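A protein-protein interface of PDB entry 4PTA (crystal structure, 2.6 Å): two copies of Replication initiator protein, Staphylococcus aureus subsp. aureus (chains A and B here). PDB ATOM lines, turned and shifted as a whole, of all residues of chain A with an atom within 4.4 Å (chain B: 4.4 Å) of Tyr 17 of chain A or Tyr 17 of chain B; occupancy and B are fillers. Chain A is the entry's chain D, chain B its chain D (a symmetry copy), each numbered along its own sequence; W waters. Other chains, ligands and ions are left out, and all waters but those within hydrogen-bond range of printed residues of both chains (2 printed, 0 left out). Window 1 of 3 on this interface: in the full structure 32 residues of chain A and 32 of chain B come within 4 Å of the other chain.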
ATOM      1  N   PHE A  16      -2.256  24.440   4.060  1.00  0.00           N
ATOM      2  CA  PHE A  16      -0.994  23.851   4.479  1.00  0.00           C
ATOM      3  C   PHE A  16      -1.214  22.559   5.252  1.00  0.00           C
ATOM      4  O   PHE A  16      -2.233  22.387   5.919  1.00  0.00           O
ATOM      5  CB  PHE A  16      -0.217  24.837   5.358  1.00  0.00           C
ATOM      6  CG  PHE A  16      -0.173  26.236   4.813  1.00  0.00           C
ATOM      7  CD1 PHE A  16      -1.194  27.134   5.084  1.00  0.00           C
ATOM      8  CD2 PHE A  16       0.894  26.658   4.036  1.00  0.00           C
ATOM      9  CE1 PHE A  16      -1.154  28.423   4.585  1.00  0.00           C
ATOM     10  CE2 PHE A  16       0.940  27.945   3.534  1.00  0.00           C
ATOM     11  CZ  PHE A  16      -0.090  28.829   3.806  1.00  0.00           C
ATOM     12  N   TYR A  17      -0.257  21.646   5.147  1.00  0.00           N
ATOM     13  CA  TYR A  17      -0.181  20.520   6.065  1.00  0.00           C
ATOM     14  C   TYR A  17       0.567  21.024   7.287  1.00  0.00           C
ATOM     15  O   TYR A  17       1.435  21.888   7.171  1.00  0.00           O
ATOM     16  CB  TYR A  17       0.553  19.343   5.433  1.00  0.00           C
ATOM     17  CG  TYR A  17      -0.192  18.727   4.272  1.00  0.00           C
ATOM     18  CD1 TYR A  17       0.351  18.721   2.987  1.00  0.00           C
ATOM     19  CD2 TYR A  17      -1.444  18.155   4.460  1.00  0.00           C
ATOM     20  CE1 TYR A  17      -0.337  18.151   1.925  1.00  0.00           C
ATOM     21  CE2 TYR A  17      -2.138  17.591   3.408  1.00  0.00           C
ATOM     22  CZ  TYR A  17      -1.584  17.592   2.146  1.00  0.00           C
ATOM     23  OH  TYR A  17      -2.286  17.027   1.108  1.00  0.00           O
ATOM     24  N   GLN A  18       0.221  20.509   8.460  1.00  0.00           N
ATOM     25  CA  GLN A  18       0.814  21.010   9.692  1.00  0.00           C
ATOM     26  C   GLN A  18       1.945  20.120  10.200  1.00  0.00           C
ATOM     27  O   GLN A  18       1.712  18.995  10.639  1.00  0.00           O
ATOM     28  CB  GLN A  18      -0.258  21.192  10.764  1.00  0.00           C
ATOM     29  CG  GLN A  18      -1.238  22.313  10.459  1.00  0.00           C
ATOM     30  CD  GLN A  18      -2.202  22.567  11.602  1.00  0.00           C
ATOM     31  OE1 GLN A  18      -3.053  21.732  11.911  1.00  0.00           O
ATOM     32  NE2 GLN A  18      -2.071  23.725  12.242  1.00  0.00           N
ATOM     33  N   LEU A  19       3.169  20.635  10.124  1.00  0.00           N
ATOM     34  CA  LEU A  19       4.354  19.935  10.617  1.00  0.00           C
ATOM     35  C   LEU A  19       4.640  20.310  12.068  1.00  0.00           C
ATOM     36  O   LEU A  19       5.009  21.441  12.357  1.00  0.00           O
ATOM     37  CB  LEU A  19       5.573  20.305   9.772  1.00  0.00           C
ATOM     38  CG  LEU A  19       6.158  19.309   8.773  1.00  0.00           C
ATOM     39  CD1 LEU A  19       7.438  19.885   8.190  1.00  0.00           C
ATOM     40  CD2 LEU A  19       6.430  17.978   9.433  1.00  0.00           C
ATOM     41  N   LYS A  21       6.449  21.287  15.105  1.00  0.00           N
ATOM     42  CA  LYS A  21       7.782  21.854  15.258  1.00  0.00           C
ATOM     43  C   LYS A  21       8.641  21.009  16.196  1.00  0.00           C
ATOM     44  O   LYS A  21       9.869  21.061  16.140  1.00  0.00           O
ATOM     45  CB  LYS A  21       7.708  23.288  15.783  1.00  0.00           C
ATOM     46  CG  LYS A  21       7.098  24.289  14.821  1.00  0.00           C
ATOM     47  CD  LYS A  21       7.170  25.695  15.395  1.00  0.00           C
ATOM     48  CE  LYS A  21       6.390  26.681  14.557  1.00  0.00           C
ATOM     49  NZ  LYS A  21       6.536  28.057  15.105  1.00  0.00           N
ATOM     50  N   PHE A  24      11.508  18.725  15.287  1.00  0.00           N
ATOM     51  CA  PHE A  24      12.787  19.322  14.933  1.00  0.00           C
ATOM     52  C   PHE A  24      13.559  19.803  16.159  1.00  0.00           C
ATOM     53  O   PHE A  24      14.538  20.537  16.041  1.00  0.00           O
ATOM     54  CB  PHE A  24      12.569  20.459  13.929  1.00  0.00           C
ATOM     55  CG  PHE A  24      11.847  20.023  12.682  1.00  0.00           C
ATOM     56  CD1 PHE A  24      10.464  19.965  12.651  1.00  0.00           C
ATOM     57  CD2 PHE A  24      12.553  19.649  11.551  1.00  0.00           C
ATOM     58  CE1 PHE A  24       9.803  19.549  11.522  1.00  0.00           C
ATOM     59  CE2 PHE A  24      11.894  19.236  10.418  1.00  0.00           C
ATOM     60  CZ  PHE A  24      10.519  19.184  10.403  1.00  0.00           C
ATOM     61  N   ALA A  41       2.302  14.683   8.983  1.00  0.00           N
ATOM     62  CA  ALA A  41       1.574  15.915   8.681  1.00  0.00           C
ATOM     63  C   ALA A  41       0.407  15.678   7.730  1.00  0.00           C
ATOM     64  O   ALA A  41      -0.681  16.217   7.934  1.00  0.00           O
ATOM     65  CB  ALA A  41       2.519  16.971   8.111  1.00  0.00           C
ATOM     66  N   ILE A  42       0.641  14.882   6.691  1.00  0.00           N
ATOM     67  CA  ILE A  42      -0.406  14.566   5.723  1.00  0.00           C
ATOM     68  C   ILE A  42      -1.564  13.812   6.378  1.00  0.00           C
ATOM     69  O   ILE A  42      -2.726  14.162   6.188  1.00  0.00           O
ATOM     70  CB  ILE A  42       0.142  13.760   4.513  1.00  0.00           C
ATOM     71  CG1 ILE A  42       1.076  14.630   3.668  1.00  0.00           C
ATOM     72  CG2 ILE A  42      -1.001  13.228   3.656  1.00  0.00           C
ATOM     73  CD1 ILE A  42       1.479  14.003   2.345  1.00  0.00           C
ATOM     74  N   ASP A  45      -3.833  15.815   8.694  1.00  0.00           N
ATOM     75  CA  ASP A  45      -4.819  16.606   7.987  1.00  0.00           C
ATOM     76  C   ASP A  45      -6.114  15.831   7.736  1.00  0.00           C
ATOM     77  O   ASP A  45      -7.159  16.434   7.503  1.00  0.00           O
ATOM     78  CB  ASP A  45      -4.230  17.107   6.665  1.00  0.00           C
ATOM     79  CG  ASP A  45      -5.034  18.246   6.060  1.00  0.00           C
ATOM     80  OD1 ASP A  45      -5.492  19.128   6.822  1.00  0.00           O
ATOM     81  OD2 ASP A  45      -5.209  18.254   4.825  1.00  0.00           O
ATOM     82  N   ALA A 126      14.165  28.398  18.542  1.00  0.00           N
ATOM     83  CA  ALA A 126      13.893  28.183  17.126  1.00  0.00           C
ATOM     84  C   ALA A 126      12.917  29.211  16.552  1.00  0.00           C
ATOM     85  O   ALA A 126      12.897  29.448  15.344  1.00  0.00           O
ATOM     86  CB  ALA A 126      13.371  26.772  16.900  1.00  0.00           C
ATOM     87  N   PHE B  16       3.069  24.317  14.733  1.00  0.00           N
ATOM     88  CA  PHE B  16       3.399  23.612  13.504  1.00  0.00           C
ATOM     89  C   PHE B  16       4.075  24.534  12.500  1.00  0.00           C
ATOM     90  O   PHE B  16       3.823  25.738  12.479  1.00  0.00           O
ATOM     91  CB  PHE B  16       2.131  23.025  12.875  1.00  0.00           C
ATOM     92  CG  PHE B  16       1.237  22.316  13.852  1.00  0.00           C
ATOM     93  CD1 PHE B  16       0.290  23.018  14.582  1.00  0.00           C
ATOM     94  CD2 PHE B  16       1.337  20.946  14.036  1.00  0.00           C
ATOM     95  CE1 PHE B  16      -0.536  22.367  15.480  1.00  0.00           C
ATOM     96  CE2 PHE B  16       0.514  20.290  14.933  1.00  0.00           C
ATOM     97  CZ  PHE B  16      -0.422  21.004  15.659  1.00  0.00           C
ATOM     98  N   TYR B  17       4.944  23.963  11.676  1.00  0.00           N
ATOM     99  CA  TYR B  17       5.414  24.646  10.480  1.00  0.00           C
ATOM    100  C   TYR B  17       4.372  24.381   9.409  1.00  0.00           C
ATOM    101  O   TYR B  17       3.739  23.326   9.405  1.00  0.00           O
ATOM    102  CB  TYR B  17       6.777  24.119  10.046  1.00  0.00           C
ATOM    103  CG  TYR B  17       7.883  24.442  11.024  1.00  0.00           C
ATOM    104  CD1 TYR B  17       8.592  23.430  11.673  1.00  0.00           C
ATOM    105  CD2 TYR B  17       8.215  25.762  11.304  1.00  0.00           C
ATOM    106  CE1 TYR B  17       9.608  23.734  12.569  1.00  0.00           C
ATOM    107  CE2 TYR B  17       9.220  26.072  12.198  1.00  0.00           C
ATOM    108  CZ  TYR B  17       9.912  25.059  12.827  1.00  0.00           C
ATOM    109  OH  TYR B  17      10.910  25.384  13.714  1.00  0.00           O
ATOM    110  N   GLN B  18       4.172  25.339   8.513  1.00  0.00           N
ATOM    111  CA  GLN B  18       3.120  25.211   7.514  1.00  0.00           C
ATOM    112  C   GLN B  18       3.653  24.750   6.161  1.00  0.00           C
ATOM    113  O   GLN B  18       4.363  25.487   5.478  1.00  0.00           O
ATOM    114  CB  GLN B  18       2.352  26.524   7.377  1.00  0.00           C
ATOM    115  CG  GLN B  18       1.523  26.873   8.602  1.00  0.00           C
ATOM    116  CD  GLN B  18       0.661  28.102   8.387  1.00  0.00           C
ATOM    117  OE1 GLN B  18       1.168  29.216   8.252  1.00  0.00           O
ATOM    118  NE2 GLN B  18      -0.653  27.905   8.349  1.00  0.00           N
ATOM    119  N   LEU B  19       3.309  23.519   5.789  1.00  0.00           N
ATOM    120  CA  LEU B  19       3.691  22.946   4.500  1.00  0.00           C
ATOM    121  C   LEU B  19       2.617  23.211   3.449  1.00  0.00           C
ATOM    122  O   LEU B  19       1.521  22.670   3.530  1.00  0.00           O
ATOM    123  CB  LEU B  19       3.877  21.435   4.631  1.00  0.00           C
ATOM    124  CG  LEU B  19       5.276  20.819   4.621  1.00  0.00           C
ATOM    125  CD1 LEU B  19       5.151  19.305   4.617  1.00  0.00           C
ATOM    126  CD2 LEU B  19       6.064  21.289   3.422  1.00  0.00           C
ATOM    127  N   LYS B  21       0.257  22.682   0.692  1.00  0.00           N
ATOM    128  CA  LYS B  21      -0.248  21.442   0.118  1.00  0.00           C
ATOM    129  C   LYS B  21       0.008  21.382  -1.386  1.00  0.00           C
ATOM    130  O   LYS B  21       0.045  20.302  -1.973  1.00  0.00           O
ATOM    131  CB  LYS B  21      -1.744  21.284   0.391  1.00  0.00           C
ATOM    132  CG  LYS B  21      -2.108  21.074   1.849  1.00  0.00           C
ATOM    133  CD  LYS B  21      -3.600  20.821   1.996  1.00  0.00           C
ATOM    134  CE  LYS B  21      -4.024  20.813   3.446  1.00  0.00           C
ATOM    135  NZ  LYS B  21      -5.473  20.496   3.561  1.00  0.00           N
ATOM    136  N   PHE B  24       2.546  19.275  -3.225  1.00  0.00           N
ATOM    137  CA  PHE B  24       2.282  17.853  -3.386  1.00  0.00           C
ATOM    138  C   PHE B  24       1.258  17.577  -4.485  1.00  0.00           C
ATOM    139  O   PHE B  24       0.740  16.468  -4.601  1.00  0.00           O
ATOM    140  CB  PHE B  24       1.842  17.250  -2.048  1.00  0.00           C
ATOM    141  CG  PHE B  24       2.841  17.461  -0.942  1.00  0.00           C
ATOM    142  CD1 PHE B  24       2.848  18.637  -0.212  1.00  0.00           C
ATOM    143  CD2 PHE B  24       3.788  16.494  -0.650  1.00  0.00           C
ATOM    144  CE1 PHE B  24       3.771  18.841   0.784  1.00  0.00           C
ATOM    145  CE2 PHE B  24       4.709  16.692   0.348  1.00  0.00           C
ATOM    146  CZ  PHE B  24       4.703  17.866   1.066  1.00  0.00           C
ATOM    147  N   ALA B  41       8.917  25.619   4.520  1.00  0.00           N
ATOM    148  CA  ALA B  41       8.003  25.721   5.657  1.00  0.00           C
ATOM    149  C   ALA B  41       8.658  26.374   6.868  1.00  0.00           C
ATOM    150  O   ALA B  41       8.048  27.215   7.528  1.00  0.00           O
ATOM    151  CB  ALA B  41       7.451  24.347   6.027  1.00  0.00           C
ATOM    152  N   ILE B  42       9.893  25.977   7.161  1.00  0.00           N
ATOM    153  CA  ILE B  42      10.630  26.545   8.286  1.00  0.00           C
ATOM    154  C   ILE B  42      10.872  28.043   8.097  1.00  0.00           C
ATOM    155  O   ILE B  42      10.626  28.837   9.003  1.00  0.00           O
ATOM    156  CB  ILE B  42      11.977  25.812   8.534  1.00  0.00           C
ATOM    157  CG1 ILE B  42      11.727  24.386   9.030  1.00  0.00           C
ATOM    158  CG2 ILE B  42      12.832  26.577   9.536  1.00  0.00           C
ATOM    159  CD1 ILE B  42      12.977  23.670   9.513  1.00  0.00           C
ATOM    160  N   ASP B  45       7.851  30.338   8.469  1.00  0.00           N
ATOM    161  CA  ASP B  45       7.514  30.622   9.849  1.00  0.00           C
ATOM    162  C   ASP B  45       8.248  31.852  10.385  1.00  0.00           C
ATOM    163  O   ASP B  45       7.817  32.449  11.369  1.00  0.00           O
ATOM    164  CB  ASP B  45       7.815  29.397  10.719  1.00  0.00           C
ATOM    165  CG  ASP B  45       7.136  29.463  12.077  1.00  0.00           C
ATOM    166  OD1 ASP B  45       5.966  29.904  12.143  1.00  0.00           O
ATOM    167  OD2 ASP B  45       7.777  29.076  13.075  1.00  0.00           O
ATOM    168  N   ALA B 126      -7.259  15.408  -2.847  1.00  0.00           N
ATOM    169  CA  ALA B 126      -6.338  15.096  -1.760  1.00  0.00           C
ATOM    170  C   ALA B 126      -6.946  15.355  -0.381  1.00  0.00           C
ATOM    171  O   ALA B 126      -6.507  14.778   0.613  1.00  0.00           O
ATOM    172  CB  ALA B 126      -5.045  15.882  -1.926  1.00  0.00           C
HETATM  173  O   HOH W   1      11.905  23.622  15.871  1.00  0.00           O
HETATM  174  O   HOH W   2      -1.894  17.663  -1.753  1.00  0.00           O
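Tyr 17 of chain A touches five residues of chain B.
Tyr 17 of chain B touches five residues of chain A.
Of the printed residues of chain A, Leu 19 of chain B touches Phe 16 and Tyr 17.
Of the printed residues of chain A, Lys 21 of chain B touches Phe 16 (3.4 Å), Tyr 17 (3.4 Å) and Asp 45 (2.6 Å).
Printed residues of chain A within 4 Å of Phe 24 of chain B: Tyr 17 (3.9 Å).
Ala 126 of chain B touches none of the printed residues of chain A.
The nearest printed residue of chain B that does not touch Phe 24 of chain A is Ile 42 of chain B (4.5 Å).
O of Leu 19 of chain B is in hydrogen-bond range of N of Tyr 17 of chain A (2.6 Å).
N of Tyr 17 of chain B is in hydrogen-bond range of O of Leu 19 of chain A (2.6 Å).
OD2 of Asp 45 of chain A is in salt-bridge range of NZ of Lys 21 of chain B, 2.6 Å away.
The side-chain amino group (NZ) of Lys 21 of chain A is in salt-bridge range of the side-chain carboxylate (OD2) of Asp 45 of chain B, 2.6 Å away.
Gln 18 of chain B touches Phe 16 of chain A.
O of Phe 16 of chain A touches CE of Lys 21 of chain B (3.4 Å).
Tyr 17 of chain B touches Tyr 17 of chain A.
CA of Gln 18 of chain B touches O of Tyr 17 of chain A, at 3.7 Å.
Tyr 17 of chain A touches Phe 24 of chain B.
Gln 18 of chain A touches Phe 16 of chain B.
CA of Gln 18 of chain A touches O of Tyr 17 of chain B, 3.7 Å away.
Leu 19 of chain A touches Phe 16 of chain B (O to CA, 2.9 Å).
Phe 16 of chain B touches Lys 21 of chain A.
Tyr 17 of chain B touches Lys 21 of chain A.
Phe 16 of chain A touches Gln 18 of chain B, and with the chains exchanged Gln 18 of chain A touches Phe 16 of chain B.
Phe 16 of chain A touches Lys 21 of chain B, and with the chains exchanged Lys 21 of chain A touches Phe 16 of chain B.
Tyr 17 of chain A touches its own counterpart, Tyr 17 of chain B.
Tyr 17 of chain A touches Lys 21 of chain B, and with the chains exchanged Lys 21 of chain A touches Tyr 17 of chain B.
Positions printed for both chains: 16, 17, 18, 19, 21, 24, 41, 42, 45 and 126.
Of the 17 pairs that touch across the chains among the printed residues, 17 have their exchanged pair printed and touching as well.
Water W2 bridges OH of Tyr 17 of chain A (3.0 Å) and O of Lys 21 of chain B (3.3 Å).
Water W1 bridges OH of Tyr 17 of chain B (3.0 Å) and O of Lys 21 of chain A (3.3 Å).
Printed residues of chain A that touch a printed residue of chain B: Phe 16, Tyr 17, Gln 18, Leu 19, Lys 21, Phe 24 and Asp 45.
Hydrophobic or aromatic side chains of chain A that line the printed part of chain B: Phe 16, Tyr 17, Leu 19 and Phe 24.
Among the printed residues, Asp or Glu carboxylates within 4 Å of a Lys or Arg side-chain nitrogen of the other chain: Lys 21 of chain A with Asp 45 of chain B (2.6 Å) and Asp 45 of chain A with Lys 21 of chain B (2.6 Å).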
